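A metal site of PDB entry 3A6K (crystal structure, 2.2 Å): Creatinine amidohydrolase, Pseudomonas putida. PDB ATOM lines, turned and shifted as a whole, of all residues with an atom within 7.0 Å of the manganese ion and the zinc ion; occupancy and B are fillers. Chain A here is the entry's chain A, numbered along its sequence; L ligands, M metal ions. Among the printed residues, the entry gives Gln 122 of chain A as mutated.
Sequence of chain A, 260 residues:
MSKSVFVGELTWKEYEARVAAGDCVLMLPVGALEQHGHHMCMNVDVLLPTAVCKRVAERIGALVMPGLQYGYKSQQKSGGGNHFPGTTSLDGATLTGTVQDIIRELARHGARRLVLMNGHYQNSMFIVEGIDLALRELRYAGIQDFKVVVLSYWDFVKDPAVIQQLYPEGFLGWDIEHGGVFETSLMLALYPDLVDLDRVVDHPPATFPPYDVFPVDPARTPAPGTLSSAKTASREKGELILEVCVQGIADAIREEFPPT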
ATOM      1  N   GLY A  31      37.466  -0.604  16.956  1.00  0.00           N
ATOM      2  CA  GLY A  31      36.327  -1.482  16.761  1.00  0.00           C
ATOM      3  C   GLY A  31      36.345  -2.805  17.501  1.00  0.00           C
ATOM      4  O   GLY A  31      36.747  -2.868  18.671  1.00  0.00           O
ATOM      5  N   ALA A  32      35.911  -3.852  16.823  1.00  0.00           N
ATOM      6  CA  ALA A  32      35.866  -5.187  17.409  1.00  0.00           C
ATOM      7  C   ALA A  32      35.505  -6.262  16.387  1.00  0.00           C
ATOM      8  O   ALA A  32      34.971  -5.953  15.312  1.00  0.00           O
ATOM      9  CB  ALA A  32      34.851  -5.217  18.559  1.00  0.00           C
ATOM     10  N   GLU A  34      33.104  -8.968  16.350  1.00  0.00           N
ATOM     11  CA  GLU A  34      31.965  -9.422  17.137  1.00  0.00           C
ATOM     12  C   GLU A  34      30.783  -9.911  16.290  1.00  0.00           C
ATOM     13  O   GLU A  34      30.526  -9.396  15.201  1.00  0.00           O
ATOM     14  CB  GLU A  34      31.543  -8.251  18.022  1.00  0.00           C
ATOM     15  CG  GLU A  34      30.423  -8.496  18.989  1.00  0.00           C
ATOM     16  CD  GLU A  34      30.005  -7.197  19.652  1.00  0.00           C
ATOM     17  OE1 GLU A  34      29.904  -6.184  18.928  1.00  0.00           O
ATOM     18  OE2 GLU A  34      29.775  -7.186  20.871  1.00  0.00           O
ATOM     19  N   GLN A  35      30.056 -10.898  16.800  1.00  0.00           N
ATOM     20  CA  GLN A  35      28.914 -11.415  16.068  1.00  0.00           C
ATOM     21  C   GLN A  35      27.876 -10.320  15.886  1.00  0.00           C
ATOM     22  O   GLN A  35      27.652  -9.498  16.771  1.00  0.00           O
ATOM     23  CB  GLN A  35      28.297 -12.633  16.778  1.00  0.00           C
ATOM     24  CG  GLN A  35      27.626 -12.387  18.121  1.00  0.00           C
ATOM     25  CD  GLN A  35      26.275 -11.702  17.995  1.00  0.00           C
ATOM     26  OE1 GLN A  35      25.573 -11.868  17.003  1.00  0.00           O
ATOM     27  NE2 GLN A  35      25.907 -10.931  19.019  1.00  0.00           N
ATOM     28  N   HIS A  36      27.254 -10.294  14.705  1.00  0.00           N
ATOM     29  CA  HIS A  36      26.235  -9.307  14.402  1.00  0.00           C
ATOM     30  C   HIS A  36      24.992  -9.953  13.802  1.00  0.00           C
ATOM     31  O   HIS A  36      24.498  -9.526  12.751  1.00  0.00           O
ATOM     32  CB  HIS A  36      26.776  -8.233  13.470  1.00  0.00           C
ATOM     33  CG  HIS A  36      27.455  -7.111  14.197  1.00  0.00           C
ATOM     34  ND1 HIS A  36      28.660  -7.264  14.834  1.00  0.00           N
ATOM     35  CD2 HIS A  36      27.052  -5.845  14.435  1.00  0.00           C
ATOM     36  CE1 HIS A  36      28.973  -6.135  15.443  1.00  0.00           C
ATOM     37  NE2 HIS A  36      28.012  -5.251  15.223  1.00  0.00           N
ATOM     38  N   MET A  40      24.582  -9.845   9.219  1.00  0.00           N
ATOM     39  CA  MET A  40      25.788  -9.050   8.976  1.00  0.00           C
ATOM     40  C   MET A  40      27.078  -9.730   9.370  1.00  0.00           C
ATOM     41  O   MET A  40      27.097 -10.650  10.196  1.00  0.00           O
ATOM     42  CB  MET A  40      25.709  -7.702   9.711  1.00  0.00           C
ATOM     43  CG  MET A  40      24.648  -6.760   9.213  1.00  0.00           C
ATOM     44  SD  MET A  40      24.844  -5.114   9.917  1.00  0.00           S
ATOM     45  CE  MET A  40      24.356  -5.430  11.610  1.00  0.00           C
ATOM     46  N   VAL A  44      31.816  -5.235  11.539  1.00  0.00           N
ATOM     47  CA  VAL A  44      31.000  -4.027  11.466  1.00  0.00           C
ATOM     48  C   VAL A  44      31.543  -2.877  12.309  1.00  0.00           C
ATOM     49  O   VAL A  44      31.651  -1.748  11.836  1.00  0.00           O
ATOM     50  CB  VAL A  44      29.547  -4.319  11.928  1.00  0.00           C
ATOM     51  CG1 VAL A  44      28.768  -3.022  12.125  1.00  0.00           C
ATOM     52  CG2 VAL A  44      28.856  -5.215  10.896  1.00  0.00           C
ATOM     53  N   ASP A  45      31.884  -3.183  13.567  1.00  0.00           N
ATOM     54  CA  ASP A  45      32.401  -2.172  14.484  1.00  0.00           C
ATOM     55  C   ASP A  45      33.730  -1.554  14.091  1.00  0.00           C
ATOM     56  O   ASP A  45      34.140  -0.557  14.671  1.00  0.00           O
ATOM     57  CB  ASP A  45      32.510  -2.754  15.890  1.00  0.00           C
ATOM     58  CG  ASP A  45      31.167  -3.086  16.473  1.00  0.00           C
ATOM     59  OD1 ASP A  45      30.159  -2.857  15.773  1.00  0.00           O
ATOM     60  OD2 ASP A  45      31.106  -3.585  17.616  1.00  0.00           O
ATOM     61  N   LEU A  48      32.327   0.584  10.204  1.00  0.00           N
ATOM     62  CA  LEU A  48      31.549   1.806  10.395  1.00  0.00           C
ATOM     63  C   LEU A  48      32.367   3.000  10.894  1.00  0.00           C
ATOM     64  O   LEU A  48      32.384   4.050  10.256  1.00  0.00           O
ATOM     65  CB  LEU A  48      30.348   1.526  11.302  1.00  0.00           C
ATOM     66  CG  LEU A  48      29.348   0.498  10.738  1.00  0.00           C
ATOM     67  CD1 LEU A  48      28.117   0.426  11.620  1.00  0.00           C
ATOM     68  CD2 LEU A  48      28.952   0.897   9.327  1.00  0.00           C
ATOM     69  N   TYR A  72      37.152  -4.762  23.512  1.00  0.00           N
ATOM     70  CA  TYR A  72      36.804  -5.385  24.773  1.00  0.00           C
ATOM     71  C   TYR A  72      35.649  -6.382  24.682  1.00  0.00           C
ATOM     72  O   TYR A  72      34.807  -6.273  23.808  1.00  0.00           O
ATOM     73  CB  TYR A  72      36.451  -4.319  25.824  1.00  0.00           C
ATOM     74  CG  TYR A  72      36.315  -4.932  27.193  1.00  0.00           C
ATOM     75  CD1 TYR A  72      37.375  -5.617  27.785  1.00  0.00           C
ATOM     76  CD2 TYR A  72      35.101  -4.890  27.870  1.00  0.00           C
ATOM     77  CE1 TYR A  72      37.236  -6.250  29.002  1.00  0.00           C
ATOM     78  CE2 TYR A  72      34.952  -5.538  29.109  1.00  0.00           C
ATOM     79  CZ  TYR A  72      36.026  -6.212  29.660  1.00  0.00           C
ATOM     80  OH  TYR A  72      35.862  -6.872  30.857  1.00  0.00           O
ATOM     81  N   SER A  74      32.394  -8.671  24.886  1.00  0.00           N
ATOM     82  CA  SER A  74      30.999  -8.312  24.682  1.00  0.00           C
ATOM     83  C   SER A  74      30.165  -8.544  25.946  1.00  0.00           C
ATOM     84  O   SER A  74      30.352  -9.535  26.650  1.00  0.00           O
ATOM     85  CB  SER A  74      30.409  -9.140  23.530  1.00  0.00           C
ATOM     86  OG  SER A  74      29.031  -8.864  23.376  1.00  0.00           O
ATOM     87  N   SER A  78      24.512  -5.527  26.026  1.00  0.00           N
ATOM     88  CA  SER A  78      25.003  -4.536  25.069  1.00  0.00           C
ATOM     89  C   SER A  78      25.468  -5.117  23.735  1.00  0.00           C
ATOM     90  O   SER A  78      25.727  -4.368  22.785  1.00  0.00           O
ATOM     91  CB  SER A  78      26.140  -3.725  25.690  1.00  0.00           C
ATOM     92  OG  SER A  78      25.689  -2.978  26.808  1.00  0.00           O
ATOM     93  N   GLY A  79      25.583  -6.438  23.653  1.00  0.00           N
ATOM     94  CA  GLY A  79      26.034  -7.051  22.426  1.00  0.00           C
ATOM     95  C   GLY A  79      25.841  -8.553  22.388  1.00  0.00           C
ATOM     96  O   GLY A  79      26.606  -9.274  21.734  1.00  0.00           O
ATOM     97  N   GLY A 119      33.684   2.272  17.850  1.00  0.00           N
ATOM     98  CA  GLY A 119      32.552   1.670  17.148  1.00  0.00           C
ATOM     99  C   GLY A 119      31.948   0.524  17.939  1.00  0.00           C
ATOM    100  O   GLY A 119      30.936  -0.054  17.532  1.00  0.00           O
ATOM    101  N   HIS A 120      32.560   0.196  19.063  1.00  0.00           N
ATOM    102  CA  HIS A 120      32.122  -0.909  19.927  1.00  0.00           C
ATOM    103  C   HIS A 120      31.853  -0.342  21.320  1.00  0.00           C
ATOM    104  O   HIS A 120      32.772   0.054  22.036  1.00  0.00           O
ATOM    105  CB  HIS A 120      33.223  -1.983  19.951  1.00  0.00           C
ATOM    106  CG  HIS A 120      32.901  -3.183  20.792  1.00  0.00           C
ATOM    107  ND1 HIS A 120      31.761  -3.941  20.616  1.00  0.00           N
ATOM    108  CD2 HIS A 120      33.614  -3.809  21.756  1.00  0.00           C
ATOM    109  CE1 HIS A 120      31.783  -4.969  21.432  1.00  0.00           C
ATOM    110  NE2 HIS A 120      32.893  -4.910  22.145  1.00  0.00           N
ATOM    111  N   TYR A 121      30.572  -0.281  21.670  1.00  0.00           N
ATOM    112  CA  TYR A 121      30.084   0.246  22.949  1.00  0.00           C
ATOM    113  C   TYR A 121      30.940  -0.070  24.187  1.00  0.00           C
ATOM    114  O   TYR A 121      31.228   0.810  25.006  1.00  0.00           O
ATOM    115  CB  TYR A 121      28.651  -0.233  23.183  1.00  0.00           C
ATOM    116  CG  TYR A 121      28.007   0.301  24.453  1.00  0.00           C
ATOM    117  CD1 TYR A 121      27.779   1.670  24.619  1.00  0.00           C
ATOM    118  CD2 TYR A 121      27.671  -0.557  25.504  1.00  0.00           C
ATOM    119  CE1 TYR A 121      27.222   2.174  25.797  1.00  0.00           C
ATOM    120  CE2 TYR A 121      27.111  -0.063  26.683  1.00  0.00           C
ATOM    121  CZ  TYR A 121      26.896   1.300  26.832  1.00  0.00           C
ATOM    122  OH  TYR A 121      26.357   1.786  28.006  1.00  0.00           O
ATOM    123  N   GLN A 122      31.334  -1.325  24.318  1.00  0.00           N
ATOM    124  CA  GLN A 122      32.124  -1.804  25.452  1.00  0.00           C
ATOM    125  C   GLN A 122      33.575  -1.302  25.579  1.00  0.00           C
ATOM    126  O   GLN A 122      34.175  -1.421  26.651  1.00  0.00           O
ATOM    127  CB  GLN A 122      32.147  -3.337  25.458  1.00  0.00           C
ATOM    128  CG  GLN A 122      30.819  -4.013  25.821  1.00  0.00           C
ATOM    129  CD  GLN A 122      29.861  -4.185  24.640  1.00  0.00           C
ATOM    130  OE1 GLN A 122      28.871  -4.901  24.740  1.00  0.00           O
ATOM    131  NE2 GLN A 122      30.156  -3.525  23.518  1.00  0.00           N
ATOM    132  N   ASN A 123      34.137  -0.742  24.514  1.00  0.00           N
ATOM    133  CA  ASN A 123      35.521  -0.251  24.549  1.00  0.00           C
ATOM    134  C   ASN A 123      35.741   1.009  25.353  1.00  0.00           C
ATOM    135  O   ASN A 123      36.828   1.239  25.873  1.00  0.00           O
ATOM    136  CB  ASN A 123      36.044   0.040  23.136  1.00  0.00           C
ATOM    137  CG  ASN A 123      36.167  -1.180  22.280  1.00  0.00           C
ATOM    138  OD1 ASN A 123      36.460  -2.278  22.766  1.00  0.00           O
ATOM    139  ND2 ASN A 123      35.979  -1.003  20.981  1.00  0.00           N
ATOM    140  N   TYR A 153      30.564   7.543  17.388  1.00  0.00           N
ATOM    141  CA  TYR A 153      29.818   8.198  16.330  1.00  0.00           C
ATOM    142  C   TYR A 153      28.288   8.225  16.467  1.00  0.00           C
ATOM    143  O   TYR A 153      27.649   9.180  16.052  1.00  0.00           O
ATOM    144  CB  TYR A 153      30.211   7.605  14.964  1.00  0.00           C
ATOM    145  CG  TYR A 153      29.719   6.193  14.721  1.00  0.00           C
ATOM    146  CD1 TYR A 153      28.397   5.963  14.335  1.00  0.00           C
ATOM    147  CD2 TYR A 153      30.553   5.101  14.908  1.00  0.00           C
ATOM    148  CE1 TYR A 153      27.929   4.677  14.143  1.00  0.00           C
ATOM    149  CE2 TYR A 153      30.079   3.797  14.718  1.00  0.00           C
ATOM    150  CZ  TYR A 153      28.768   3.606  14.337  1.00  0.00           C
ATOM    151  OH  TYR A 153      28.272   2.342  14.157  1.00  0.00           O
ATOM    152  N   TRP A 154      27.718   7.189  17.067  1.00  0.00           N
ATOM    153  CA  TRP A 154      26.263   7.138  17.201  1.00  0.00           C
ATOM    154  C   TRP A 154      25.685   8.188  18.144  1.00  0.00           C
ATOM    155  O   TRP A 154      24.480   8.469  18.123  1.00  0.00           O
ATOM    156  CB  TRP A 154      25.817   5.743  17.645  1.00  0.00           C
ATOM    157  CG  TRP A 154      26.407   5.274  18.918  1.00  0.00           C
ATOM    158  CD1 TRP A 154      26.109   5.705  20.177  1.00  0.00           C
ATOM    159  CD2 TRP A 154      27.425   4.278  19.077  1.00  0.00           C
ATOM    160  NE1 TRP A 154      26.874   5.046  21.104  1.00  0.00           N
ATOM    161  CE2 TRP A 154      27.696   4.160  20.462  1.00  0.00           C
ATOM    162  CE3 TRP A 154      28.146   3.462  18.176  1.00  0.00           C
ATOM    163  CZ2 TRP A 154      28.653   3.275  20.972  1.00  0.00           C
ATOM    164  CZ3 TRP A 154      29.094   2.580  18.683  1.00  0.00           C
ATOM    165  CH2 TRP A 154      29.341   2.491  20.069  1.00  0.00           C
ATOM    166  N   GLU A 177      20.316  -1.842  20.584  1.00  0.00           N
ATOM    167  CA  GLU A 177      20.591  -1.499  19.200  1.00  0.00           C
ATOM    168  C   GLU A 177      21.789  -2.254  18.619  1.00  0.00           C
ATOM    169  O   GLU A 177      22.477  -1.742  17.730  1.00  0.00           O
ATOM    170  CB  GLU A 177      20.789   0.012  19.093  1.00  0.00           C
ATOM    171  CG  GLU A 177      20.740   0.560  17.662  1.00  0.00           C
ATOM    172  CD  GLU A 177      19.479   0.175  16.915  1.00  0.00           C
ATOM    173  OE1 GLU A 177      18.358   0.458  17.405  1.00  0.00           O
ATOM    174  OE2 GLU A 177      19.605  -0.421  15.823  1.00  0.00           O
ATOM    175  N   HIS A 178      22.037  -3.464  19.108  1.00  0.00           N
ATOM    176  CA  HIS A 178      23.147  -4.275  18.606  1.00  0.00           C
ATOM    177  C   HIS A 178      22.679  -5.086  17.410  1.00  0.00           C
ATOM    178  O   HIS A 178      21.914  -6.046  17.567  1.00  0.00           O
ATOM    179  CB  HIS A 178      23.661  -5.235  19.683  1.00  0.00           C
ATOM    180  CG  HIS A 178      24.768  -6.135  19.218  1.00  0.00           C
ATOM    181  ND1 HIS A 178      26.040  -5.670  18.969  1.00  0.00           N
ATOM    182  CD2 HIS A 178      24.783  -7.452  18.932  1.00  0.00           C
ATOM    183  CE1 HIS A 178      26.802  -6.666  18.535  1.00  0.00           C
ATOM    184  NE2 HIS A 178      26.065  -7.757  18.505  1.00  0.00           N
ATOM    185  N   GLY A 179      23.148  -4.725  16.222  1.00  0.00           N
ATOM    186  CA  GLY A 179      22.751  -5.442  15.021  1.00  0.00           C
ATOM    187  C   GLY A 179      21.353  -5.061  14.584  1.00  0.00           C
ATOM    188  O   GLY A 179      20.757  -5.691  13.703  1.00  0.00           O
ATOM    189  N   GLU A 183      22.831   0.039  12.922  1.00  0.00           N
ATOM    190  CA  GLU A 183      24.031  -0.503  12.279  1.00  0.00           C
ATOM    191  C   GLU A 183      23.749  -1.100  10.919  1.00  0.00           C
ATOM    192  O   GLU A 183      24.538  -0.933   9.991  1.00  0.00           O
ATOM    193  CB  GLU A 183      24.683  -1.557  13.150  1.00  0.00           C
ATOM    194  CG  GLU A 183      25.416  -1.013  14.342  1.00  0.00           C
ATOM    195  CD  GLU A 183      26.223  -2.090  15.028  1.00  0.00           C
ATOM    196  OE1 GLU A 183      25.627  -3.100  15.452  1.00  0.00           O
ATOM    197  OE2 GLU A 183      27.461  -1.924  15.142  1.00  0.00           O
HETATM  198 CL1  LIG L   1      27.891  -2.323  19.052  1.00  0.00          CL
HETATM  199 MN    MN M   1      29.930  -4.076  19.428  1.00  0.00          MN
HETATM  200 ZN    ZN M   2      28.169  -3.427  16.267  1.00  0.00          ZN
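OE1 of Glu 34 binds the manganese ion, at 2.2 Å. The manganese ion is bound by a ring nitrogen (ND1) of His 120, 2.2 Å away. The manganese ion is bound by the side-chain carboxylate (OD2) of Asp 45, 2.2 Å away. CL1 of the ligand is bound to the manganese ion, 2.7 Å away.
Three residues have an atom within 4 Å of the zinc ion: His 36, Asp 45 and Glu 183. The nearest printed residue that does not touch the zinc ion is His 178 (4.1 Å).
The side-chain carboxylate (OE1) of Glu 183 is in hydrogen-bond range of the backbone NH (N) of Gly 179 (3.1 Å). O of Glu 34 sits at hydrogen-bond distance from ND1 of His 36 (2.9 Å). OE2 of Glu 34 sits at hydrogen-bond distance from OG of Ser 74, 3.1 Å away. A ring nitrogen (NE2) of His 120 sits close to the side-chain amide nitrogen (NE2) of Gln 122, 3.4 Å away. O of Tyr 72 sits at hydrogen-bond distance from NE2 of His 120, at 2.9 Å.
The zinc ion is bound by the side-chain carboxylate of Glu 183 (2.0 Å), a ring nitrogen (NE2) of His 36 (2.1 Å) and the side-chain carboxylate of Asp 45 (2.1 Å). Slightly farther from the zinc ion lies OE1 of Glu 183 (2.7 Å). Slightly farther from the zinc ion lies a chlorine (CL1) of the ligand (3.0 Å).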
